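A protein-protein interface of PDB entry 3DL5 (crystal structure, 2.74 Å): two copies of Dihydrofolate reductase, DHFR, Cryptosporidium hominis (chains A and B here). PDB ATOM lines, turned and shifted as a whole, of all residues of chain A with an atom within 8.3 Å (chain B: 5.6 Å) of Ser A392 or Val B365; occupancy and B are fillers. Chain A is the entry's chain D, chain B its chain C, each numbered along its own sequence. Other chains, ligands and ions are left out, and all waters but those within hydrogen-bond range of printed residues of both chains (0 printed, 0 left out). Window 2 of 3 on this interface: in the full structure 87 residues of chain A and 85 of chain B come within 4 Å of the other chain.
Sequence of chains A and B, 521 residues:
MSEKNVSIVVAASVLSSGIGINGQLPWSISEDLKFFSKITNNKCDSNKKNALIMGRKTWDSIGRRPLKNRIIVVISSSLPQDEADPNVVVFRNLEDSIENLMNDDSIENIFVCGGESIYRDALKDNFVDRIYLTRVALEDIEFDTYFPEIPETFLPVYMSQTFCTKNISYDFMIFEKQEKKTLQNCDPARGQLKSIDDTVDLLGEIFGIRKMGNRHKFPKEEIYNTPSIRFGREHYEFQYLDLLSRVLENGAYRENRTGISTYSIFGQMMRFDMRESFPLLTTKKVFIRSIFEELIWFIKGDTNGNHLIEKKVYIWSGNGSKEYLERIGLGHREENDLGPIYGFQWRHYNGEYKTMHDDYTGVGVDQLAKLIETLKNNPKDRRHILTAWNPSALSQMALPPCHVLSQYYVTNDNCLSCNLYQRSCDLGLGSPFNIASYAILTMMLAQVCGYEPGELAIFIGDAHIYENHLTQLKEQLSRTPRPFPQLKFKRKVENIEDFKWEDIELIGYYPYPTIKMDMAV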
ATOM      1  N   PRO A 340      -5.863  32.412   5.530  1.00  0.00           N
ATOM      2  CA  PRO A 340      -5.403  31.147   6.114  1.00  0.00           C
ATOM      3  C   PRO A 340      -4.718  31.361   7.461  1.00  0.00           C
ATOM      4  O   PRO A 340      -3.519  31.116   7.587  1.00  0.00           O
ATOM      5  CB  PRO A 340      -4.392  30.641   5.084  1.00  0.00           C
ATOM      6  CG  PRO A 340      -3.874  31.874   4.436  1.00  0.00           C
ATOM      7  CD  PRO A 340      -5.031  32.831   4.389  1.00  0.00           C
ATOM      8  N   GLN A 345      -4.503  26.907   9.399  1.00  0.00           N
ATOM      9  CA  GLN A 345      -3.216  26.221   9.481  1.00  0.00           C
ATOM     10  C   GLN A 345      -3.302  24.979  10.365  1.00  0.00           C
ATOM     11  O   GLN A 345      -2.602  24.002  10.128  1.00  0.00           O
ATOM     12  CB  GLN A 345      -2.128  27.163  10.003  1.00  0.00           C
ATOM     13  CG  GLN A 345      -1.794  28.337   9.090  1.00  0.00           C
ATOM     14  CD  GLN A 345      -1.463  27.914   7.666  1.00  0.00           C
ATOM     15  OE1 GLN A 345      -0.683  26.984   7.437  1.00  0.00           O
ATOM     16  NE2 GLN A 345      -2.054  28.608   6.697  1.00  0.00           N
ATOM     17  N   TYR A 349      -3.058  22.947   7.169  1.00  0.00           N
ATOM     18  CA  TYR A 349      -1.727  23.506   6.969  1.00  0.00           C
ATOM     19  C   TYR A 349      -1.235  23.265   5.546  1.00  0.00           C
ATOM     20  O   TYR A 349      -1.280  22.141   5.046  1.00  0.00           O
ATOM     21  CB  TYR A 349      -0.739  22.911   7.975  1.00  0.00           C
ATOM     22  CG  TYR A 349       0.591  23.627   8.023  1.00  0.00           C
ATOM     23  CD1 TYR A 349       0.809  24.668   8.916  1.00  0.00           C
ATOM     24  CD2 TYR A 349       1.630  23.262   7.177  1.00  0.00           C
ATOM     25  CE1 TYR A 349       2.024  25.326   8.964  1.00  0.00           C
ATOM     26  CE2 TYR A 349       2.848  23.914   7.218  1.00  0.00           C
ATOM     27  CZ  TYR A 349       3.040  24.945   8.112  1.00  0.00           C
ATOM     28  OH  TYR A 349       4.250  25.596   8.157  1.00  0.00           O
ATOM     29  N   ASN A 350      -0.768  24.327   4.899  1.00  0.00           N
ATOM     30  CA  ASN A 350      -0.260  24.231   3.535  1.00  0.00           C
ATOM     31  C   ASN A 350      -1.376  23.998   2.522  1.00  0.00           C
ATOM     32  O   ASN A 350      -1.119  23.624   1.377  1.00  0.00           O
ATOM     33  CB  ASN A 350       0.788  23.121   3.429  1.00  0.00           C
ATOM     34  CG  ASN A 350       2.204  23.658   3.408  1.00  0.00           C
ATOM     35  OD1 ASN A 350       2.442  24.803   3.019  1.00  0.00           O
ATOM     36  ND2 ASN A 350       3.156  22.834   3.828  1.00  0.00           N
ATOM     37  N   GLY A 351      -2.614  24.220   2.950  1.00  0.00           N
ATOM     38  CA  GLY A 351      -3.762  24.083   2.070  1.00  0.00           C
ATOM     39  C   GLY A 351      -3.802  25.353   1.240  1.00  0.00           C
ATOM     40  O   GLY A 351      -3.386  26.408   1.720  1.00  0.00           O
ATOM     41  N   TRP A 389       3.018  28.828  11.972  1.00  0.00           N
ATOM     42  CA  TRP A 389       3.907  29.643  11.156  1.00  0.00           C
ATOM     43  C   TRP A 389       4.214  29.013   9.805  1.00  0.00           C
ATOM     44  O   TRP A 389       5.012  28.076   9.703  1.00  0.00           O
ATOM     45  CB  TRP A 389       5.204  29.936  11.916  1.00  0.00           C
ATOM     46  CG  TRP A 389       5.956  31.070  11.324  1.00  0.00           C
ATOM     47  CD1 TRP A 389       6.976  30.996  10.429  1.00  0.00           C
ATOM     48  CD2 TRP A 389       5.674  32.464  11.502  1.00  0.00           C
ATOM     49  NE1 TRP A 389       7.347  32.259  10.027  1.00  0.00           N
ATOM     50  CE2 TRP A 389       6.563  33.179  10.670  1.00  0.00           C
ATOM     51  CE3 TRP A 389       4.748  33.178  12.280  1.00  0.00           C
ATOM     52  CZ2 TRP A 389       6.558  34.577  10.592  1.00  0.00           C
ATOM     53  CZ3 TRP A 389       4.741  34.575  12.201  1.00  0.00           C
ATOM     54  CH2 TRP A 389       5.644  35.256  11.362  1.00  0.00           C
ATOM     55  N   ASN A 390       3.564  29.532   8.768  1.00  0.00           N
ATOM     56  CA  ASN A 390       3.752  29.033   7.415  1.00  0.00           C
ATOM     57  C   ASN A 390       4.229  30.182   6.542  1.00  0.00           C
ATOM     58  O   ASN A 390       3.429  31.027   6.131  1.00  0.00           O
ATOM     59  CB  ASN A 390       2.435  28.491   6.858  1.00  0.00           C
ATOM     60  CG  ASN A 390       2.624  27.695   5.578  1.00  0.00           C
ATOM     61  OD1 ASN A 390       3.521  27.975   4.776  1.00  0.00           O
ATOM     62  ND2 ASN A 390       1.764  26.705   5.372  1.00  0.00           N
ATOM     63  N   PRO A 391       5.543  30.235   6.252  1.00  0.00           N
ATOM     64  CA  PRO A 391       6.144  31.285   5.423  1.00  0.00           C
ATOM     65  C   PRO A 391       5.383  31.544   4.121  1.00  0.00           C
ATOM     66  O   PRO A 391       5.190  32.689   3.715  1.00  0.00           O
ATOM     67  CB  PRO A 391       7.556  30.756   5.185  1.00  0.00           C
ATOM     68  CG  PRO A 391       7.867  30.102   6.482  1.00  0.00           C
ATOM     69  CD  PRO A 391       6.585  29.334   6.778  1.00  0.00           C
ATOM     70  N   SER A 392       4.941  30.474   3.477  1.00  0.00           N
ATOM     71  CA  SER A 392       4.207  30.605   2.228  1.00  0.00           C
ATOM     72  C   SER A 392       2.845  31.303   2.343  1.00  0.00           C
ATOM     73  O   SER A 392       2.360  31.890   1.376  1.00  0.00           O
ATOM     74  CB  SER A 392       4.020  29.224   1.601  1.00  0.00           C
ATOM     75  OG  SER A 392       5.271  28.672   1.225  1.00  0.00           O
ATOM     76  N   ALA A 393       2.230  31.262   3.520  1.00  0.00           N
ATOM     77  CA  ALA A 393       0.914  31.873   3.693  1.00  0.00           C
ATOM     78  C   ALA A 393       0.872  33.243   4.381  1.00  0.00           C
ATOM     79  O   ALA A 393      -0.144  33.928   4.334  1.00  0.00           O
ATOM     80  CB  ALA A 393       0.008  30.899   4.434  1.00  0.00           C
ATOM     81  N   LEU A 394       1.970  33.640   5.009  1.00  0.00           N
ATOM     82  CA  LEU A 394       2.045  34.906   5.733  1.00  0.00           C
ATOM     83  C   LEU A 394       1.468  36.146   5.060  1.00  0.00           C
ATOM     84  O   LEU A 394       0.974  37.044   5.740  1.00  0.00           O
ATOM     85  CB  LEU A 394       3.493  35.197   6.106  1.00  0.00           C
ATOM     86  CG  LEU A 394       4.196  34.151   6.963  1.00  0.00           C
ATOM     87  CD1 LEU A 394       5.629  34.614   7.232  1.00  0.00           C
ATOM     88  CD2 LEU A 394       3.421  33.951   8.275  1.00  0.00           C
ATOM     89  N   SER A 395       1.544  36.207   3.735  1.00  0.00           N
ATOM     90  CA  SER A 395       1.045  37.366   2.994  1.00  0.00           C
ATOM     91  C   SER A 395      -0.476  37.465   2.910  1.00  0.00           C
ATOM     92  O   SER A 395      -1.024  38.562   2.808  1.00  0.00           O
ATOM     93  CB  SER A 395       1.622  37.358   1.579  1.00  0.00           C
ATOM     94  OG  SER A 395       1.389  36.102   0.964  1.00  0.00           O
ATOM     95  N   GLN A 396      -1.154  36.325   2.963  1.00  0.00           N
ATOM     96  CA  GLN A 396      -2.609  36.292   2.862  1.00  0.00           C
ATOM     97  C   GLN A 396      -3.312  36.429   4.206  1.00  0.00           C
ATOM     98  O   GLN A 396      -4.542  36.472   4.267  1.00  0.00           O
ATOM     99  CB  GLN A 396      -3.056  34.986   2.209  1.00  0.00           C
ATOM    100  CG  GLN A 396      -2.246  34.583   0.994  1.00  0.00           C
ATOM    101  CD  GLN A 396      -2.718  33.265   0.395  1.00  0.00           C
ATOM    102  OE1 GLN A 396      -2.618  32.201   1.020  1.00  0.00           O
ATOM    103  NE2 GLN A 396      -3.240  33.332  -0.822  1.00  0.00           N
ATOM    104  N   MET A 397      -2.541  36.500   5.284  1.00  0.00           N
ATOM    105  CA  MET A 397      -3.138  36.605   6.606  1.00  0.00           C
ATOM    106  C   MET A 397      -3.426  38.031   7.064  1.00  0.00           C
ATOM    107  O   MET A 397      -2.591  38.922   6.929  1.00  0.00           O
ATOM    108  CB  MET A 397      -2.249  35.896   7.627  1.00  0.00           C
ATOM    109  CG  MET A 397      -2.162  34.395   7.403  1.00  0.00           C
ATOM    110  SD  MET A 397      -1.099  33.556   8.588  1.00  0.00           S
ATOM    111  CE  MET A 397      -0.499  32.206   7.610  1.00  0.00           C
ATOM    112  N   GLN B 345      14.836  23.558   4.776  1.00  0.00           N
ATOM    113  CA  GLN B 345      13.725  24.387   5.230  1.00  0.00           C
ATOM    114  C   GLN B 345      14.130  25.846   5.366  1.00  0.00           C
ATOM    115  O   GLN B 345      13.353  26.741   5.051  1.00  0.00           O
ATOM    116  CB  GLN B 345      13.175  23.879   6.567  1.00  0.00           C
ATOM    117  CG  GLN B 345      12.573  22.475   6.532  1.00  0.00           C
ATOM    118  CD  GLN B 345      11.543  22.286   5.424  1.00  0.00           C
ATOM    119  OE1 GLN B 345      10.760  23.188   5.109  1.00  0.00           O
ATOM    120  NE2 GLN B 345      11.531  21.094   4.837  1.00  0.00           N
ATOM    121  N   TRP B 346      15.346  26.086   5.842  1.00  0.00           N
ATOM    122  CA  TRP B 346      15.843  27.451   6.006  1.00  0.00           C
ATOM    123  C   TRP B 346      15.891  28.203   4.675  1.00  0.00           C
ATOM    124  O   TRP B 346      15.395  29.334   4.560  1.00  0.00           O
ATOM    125  CB  TRP B 346      17.256  27.433   6.595  1.00  0.00           C
ATOM    126  CG  TRP B 346      17.335  27.155   8.063  1.00  0.00           C
ATOM    127  CD1 TRP B 346      16.347  26.660   8.874  1.00  0.00           C
ATOM    128  CD2 TRP B 346      18.488  27.330   8.896  1.00  0.00           C
ATOM    129  NE1 TRP B 346      16.819  26.515  10.161  1.00  0.00           N
ATOM    130  CE2 TRP B 346      18.129  26.918  10.202  1.00  0.00           C
ATOM    131  CE3 TRP B 346      19.793  27.792   8.663  1.00  0.00           C
ATOM    132  CZ2 TRP B 346      19.023  26.957  11.269  1.00  0.00           C
ATOM    133  CZ3 TRP B 346      20.687  27.829   9.724  1.00  0.00           C
ATOM    134  CH2 TRP B 346      20.295  27.413  11.014  1.00  0.00           C
ATOM    135  N   ARG B 347      16.492  27.567   3.670  1.00  0.00           N
ATOM    136  CA  ARG B 347      16.631  28.190   2.355  1.00  0.00           C
ATOM    137  C   ARG B 347      15.471  27.967   1.386  1.00  0.00           C
ATOM    138  O   ARG B 347      15.179  28.837   0.573  1.00  0.00           O
ATOM    139  CB  ARG B 347      17.943  27.741   1.703  1.00  0.00           C
ATOM    140  CG  ARG B 347      19.181  27.913   2.589  1.00  0.00           C
ATOM    141  CD  ARG B 347      19.153  29.238   3.345  1.00  0.00           C
ATOM    142  NE  ARG B 347      19.057  30.391   2.454  1.00  0.00           N
ATOM    143  CZ  ARG B 347      20.077  30.874   1.754  1.00  0.00           C
ATOM    144  NH1 ARG B 347      21.271  30.307   1.846  1.00  0.00           N
ATOM    145  NH2 ARG B 347      19.902  31.917   0.959  1.00  0.00           N
ATOM    146  N   HIS B 348      14.798  26.822   1.477  1.00  0.00           N
ATOM    147  CA  HIS B 348      13.681  26.523   0.578  1.00  0.00           C
ATOM    148  C   HIS B 348      12.474  25.975   1.311  1.00  0.00           C
ATOM    149  O   HIS B 348      12.068  24.844   1.071  1.00  0.00           O
ATOM    150  CB  HIS B 348      14.104  25.486  -0.453  1.00  0.00           C
ATOM    151  CG  HIS B 348      15.500  25.669  -0.945  1.00  0.00           C
ATOM    152  ND1 HIS B 348      15.848  26.648  -1.850  1.00  0.00           N
ATOM    153  CD2 HIS B 348      16.645  25.022  -0.628  1.00  0.00           C
ATOM    154  CE1 HIS B 348      17.152  26.594  -2.069  1.00  0.00           C
ATOM    155  NE2 HIS B 348      17.658  25.615  -1.340  1.00  0.00           N
ATOM    156  N   TYR B 349      11.894  26.775   2.193  1.00  0.00           N
ATOM    157  CA  TYR B 349      10.743  26.309   2.926  1.00  0.00           C
ATOM    158  C   TYR B 349       9.716  25.881   1.889  1.00  0.00           C
ATOM    159  O   TYR B 349       9.478  26.594   0.903  1.00  0.00           O
ATOM    160  CB  TYR B 349      10.157  27.431   3.780  1.00  0.00           C
ATOM    161  CG  TYR B 349       9.105  26.929   4.722  1.00  0.00           C
ATOM    162  CD1 TYR B 349       9.463  26.186   5.843  1.00  0.00           C
ATOM    163  CD2 TYR B 349       7.753  27.147   4.469  1.00  0.00           C
ATOM    164  CE1 TYR B 349       8.513  25.670   6.686  1.00  0.00           C
ATOM    165  CE2 TYR B 349       6.787  26.628   5.310  1.00  0.00           C
ATOM    166  CZ  TYR B 349       7.184  25.891   6.419  1.00  0.00           C
ATOM    167  OH  TYR B 349       6.287  25.365   7.299  1.00  0.00           O
ATOM    168  N   ASN B 350       9.115  24.717   2.106  1.00  0.00           N
ATOM    169  CA  ASN B 350       8.101  24.209   1.194  1.00  0.00           C
ATOM    170  C   ASN B 350       8.581  23.832  -0.194  1.00  0.00           C
ATOM    171  O   ASN B 350       7.779  23.745  -1.112  1.00  0.00           O
ATOM    172  CB  ASN B 350       6.951  25.205   1.055  1.00  0.00           C
ATOM    173  CG  ASN B 350       5.885  25.004   2.108  1.00  0.00           C
ATOM    174  OD1 ASN B 350       5.652  23.880   2.555  1.00  0.00           O
ATOM    175  ND2 ASN B 350       5.218  26.084   2.501  1.00  0.00           N
ATOM    176  N   GLY B 351       9.876  23.613  -0.366  1.00  0.00           N
ATOM    177  CA  GLY B 351      10.348  23.214  -1.674  1.00  0.00           C
ATOM    178  C   GLY B 351       9.963  21.758  -1.860  1.00  0.00           C
ATOM    179  O   GLY B 351       9.870  21.014  -0.883  1.00  0.00           O
ATOM    180  N   VAL B 363      13.752  27.591  -5.670  1.00  0.00           N
ATOM    181  CA  VAL B 363      12.560  26.869  -5.227  1.00  0.00           C
ATOM    182  C   VAL B 363      12.351  27.031  -3.720  1.00  0.00           C
ATOM    183  O   VAL B 363      13.309  27.068  -2.939  1.00  0.00           O
ATOM    184  CB  VAL B 363      12.612  25.352  -5.622  1.00  0.00           C
ATOM    185  CG1 VAL B 363      13.946  25.020  -6.248  1.00  0.00           C
ATOM    186  CG2 VAL B 363      12.344  24.463  -4.414  1.00  0.00           C
ATOM    187  N   GLY B 364      11.093  27.151  -3.322  1.00  0.00           N
ATOM    188  CA  GLY B 364      10.779  27.317  -1.918  1.00  0.00           C
ATOM    189  C   GLY B 364      10.999  28.735  -1.430  1.00  0.00           C
ATOM    190  O   GLY B 364      11.523  29.574  -2.159  1.00  0.00           O
ATOM    191  N   VAL B 365      10.588  29.004  -0.194  1.00  0.00           N
ATOM    192  CA  VAL B 365      10.753  30.324   0.406  1.00  0.00           C
ATOM    193  C   VAL B 365      12.097  30.430   1.118  1.00  0.00           C
ATOM    194  O   VAL B 365      12.400  29.638   2.002  1.00  0.00           O
ATOM    195  CB  VAL B 365       9.656  30.602   1.448  1.00  0.00           C
ATOM    196  CG1 VAL B 365       9.862  31.974   2.077  1.00  0.00           C
ATOM    197  CG2 VAL B 365       8.298  30.502   0.799  1.00  0.00           C
ATOM    198  N   ASP B 366      12.902  31.411   0.738  1.00  0.00           N
ATOM    199  CA  ASP B 366      14.198  31.592   1.378  1.00  0.00           C
ATOM    200  C   ASP B 366      13.996  32.444   2.631  1.00  0.00           C
ATOM    201  O   ASP B 366      13.954  33.672   2.555  1.00  0.00           O
ATOM    202  CB  ASP B 366      15.165  32.274   0.414  1.00  0.00           C
ATOM    203  CG  ASP B 366      16.601  32.231   0.895  1.00  0.00           C
ATOM    204  OD1 ASP B 366      17.492  32.475   0.055  1.00  0.00           O
ATOM    205  OD2 ASP B 366      16.845  31.963   2.097  1.00  0.00           O
ATOM    206  N   GLN B 367      13.875  31.781   3.779  1.00  0.00           N
ATOM    207  CA  GLN B 367      13.648  32.476   5.041  1.00  0.00           C
ATOM    208  C   GLN B 367      14.875  33.194   5.573  1.00  0.00           C
ATOM    209  O   GLN B 367      14.766  34.267   6.163  1.00  0.00           O
ATOM    210  CB  GLN B 367      13.184  31.501   6.125  1.00  0.00           C
ATOM    211  CG  GLN B 367      11.966  30.674   5.804  1.00  0.00           C
ATOM    212  CD  GLN B 367      11.617  29.738   6.948  1.00  0.00           C
ATOM    213  OE1 GLN B 367      11.054  30.159   7.963  1.00  0.00           O
ATOM    214  NE2 GLN B 367      11.968  28.468   6.797  1.00  0.00           N
ATOM    215  N   LYS B 370      15.267  36.377   3.746  1.00  0.00           N
ATOM    216  CA  LYS B 370      14.269  37.321   4.215  1.00  0.00           C
ATOM    217  C   LYS B 370      14.560  37.821   5.620  1.00  0.00           C
ATOM    218  O   LYS B 370      14.332  38.988   5.932  1.00  0.00           O
ATOM    219  CB  LYS B 370      12.875  36.694   4.169  1.00  0.00           C
ATOM    220  CG  LYS B 370      12.362  36.498   2.761  1.00  0.00           C
ATOM    221  CD  LYS B 370      10.905  36.102   2.753  1.00  0.00           C
ATOM    222  CE  LYS B 370      10.343  36.136   1.342  1.00  0.00           C
ATOM    223  NZ  LYS B 370       8.870  35.931   1.341  1.00  0.00           N
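OD1 of Asn B350 sits at hydrogen-bond distance from ND2 of Asn A350, 3.0 Å away.
The side-chain amide nitrogen of Asn B350 lies within hydrogen-bond range of the side-chain amide oxygen of Asn A390.
OG of Ser A392 is in hydrogen-bond range of ND2 of Asn B350, 2.9 Å away.
The side-chain hydroxyl (OH) of Tyr B349 sits close to the side-chain hydroxyl (OH) of Tyr A349, 2.2 Å away.
Tyr A349 touches its own counterpart, Tyr B349.
Asn A350 touches its own counterpart, Asn B350.
4 positions are printed for both chains.
Of the 9 pairs that touch across the chains among the printed residues, 2 have their exchanged pair printed and touching as well.
Of chain B, only Asn B350 and Val B365 come within 4 Å of Ser A392.
Val B365 touches just one residue of chain A: Ser A392 (3.6 Å).
No residue of chain A comes within 4 Å of Gly B364.
Of the printed residues of chain B, Asn A350 touches Asn B350 (3.0 Å).
Printed residues of chain A within 4 Å of Tyr B349: Tyr A349, Trp A389, Asn A390 and Pro A391.
Of the printed residues of chain B, Tyr A349 touches Tyr B349.
Of the printed residues of chain B, Pro A391 touches Tyr B349 (3.1 Å) and Gln B367 (3.5 Å).
Printed residues of chain A within 4 Å of Asn B350: Asn A350, Asn A390 and Ser A392.
Ser A395 touches none of the printed residues of chain B.
The nearest residue of chain B that does not touch Ser A392 is Tyr B349 (4.4 Å).
The nearest residue of chain A that does not touch Val B365 is Pro A391 (4.1 Å).
The nearest printed residue of chain A that does not touch Tyr B349 is Ser A392 (4.4 Å).
The backbone carbonyl oxygen (O) of Gln B345 is in hydrogen-bond range of the side-chain amide nitrogen (NE2) of Gln B367, at 2.8 Å.
The backbone carbonyl oxygen of Trp B346 is in hydrogen-bond range of the backbone NH of Gln B367, 3.0 Å away.
The side-chain amide oxygen (OE1) of Gln A345 lies within hydrogen-bond range of the side-chain amide nitrogen (ND2) of Asn A390 (3.2 Å).
OH of Tyr A349 lies within hydrogen-bond range of O of Trp A389.
ND2 of Asn A390 sits at hydrogen-bond distance from OD1 of Asn A350 (3.1 Å).
The backbone NH of Ser A392 lies within hydrogen-bond range of the side-chain amide oxygen of Asn A390 (3.2 Å).
Of the 13 printed residues of chain B, 4 touch a printed residue of chain A.
Of the 14 printed residues of chain A, 6 touch a printed residue of chain B.
Hydrophobic or aromatic side chains of chain A within 4 Å of the printed part of chain B: Tyr A349 and Pro A391.
Among the printed residues, no Asp or Glu carboxylate lies within 4 Å of a Lys or Arg side-chain nitrogen of the other chain.
Trp A389 touches Tyr B349.
Asn A390 touches Tyr B349.
CD of Pro A391 touches CE2 of Tyr B349, 3.1 Å away.
CG of Pro A391 touches OE1 of Gln B367 (3.5 Å).
CG2 of Val B365 touches OG of Ser A392, 3.6 Å away.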
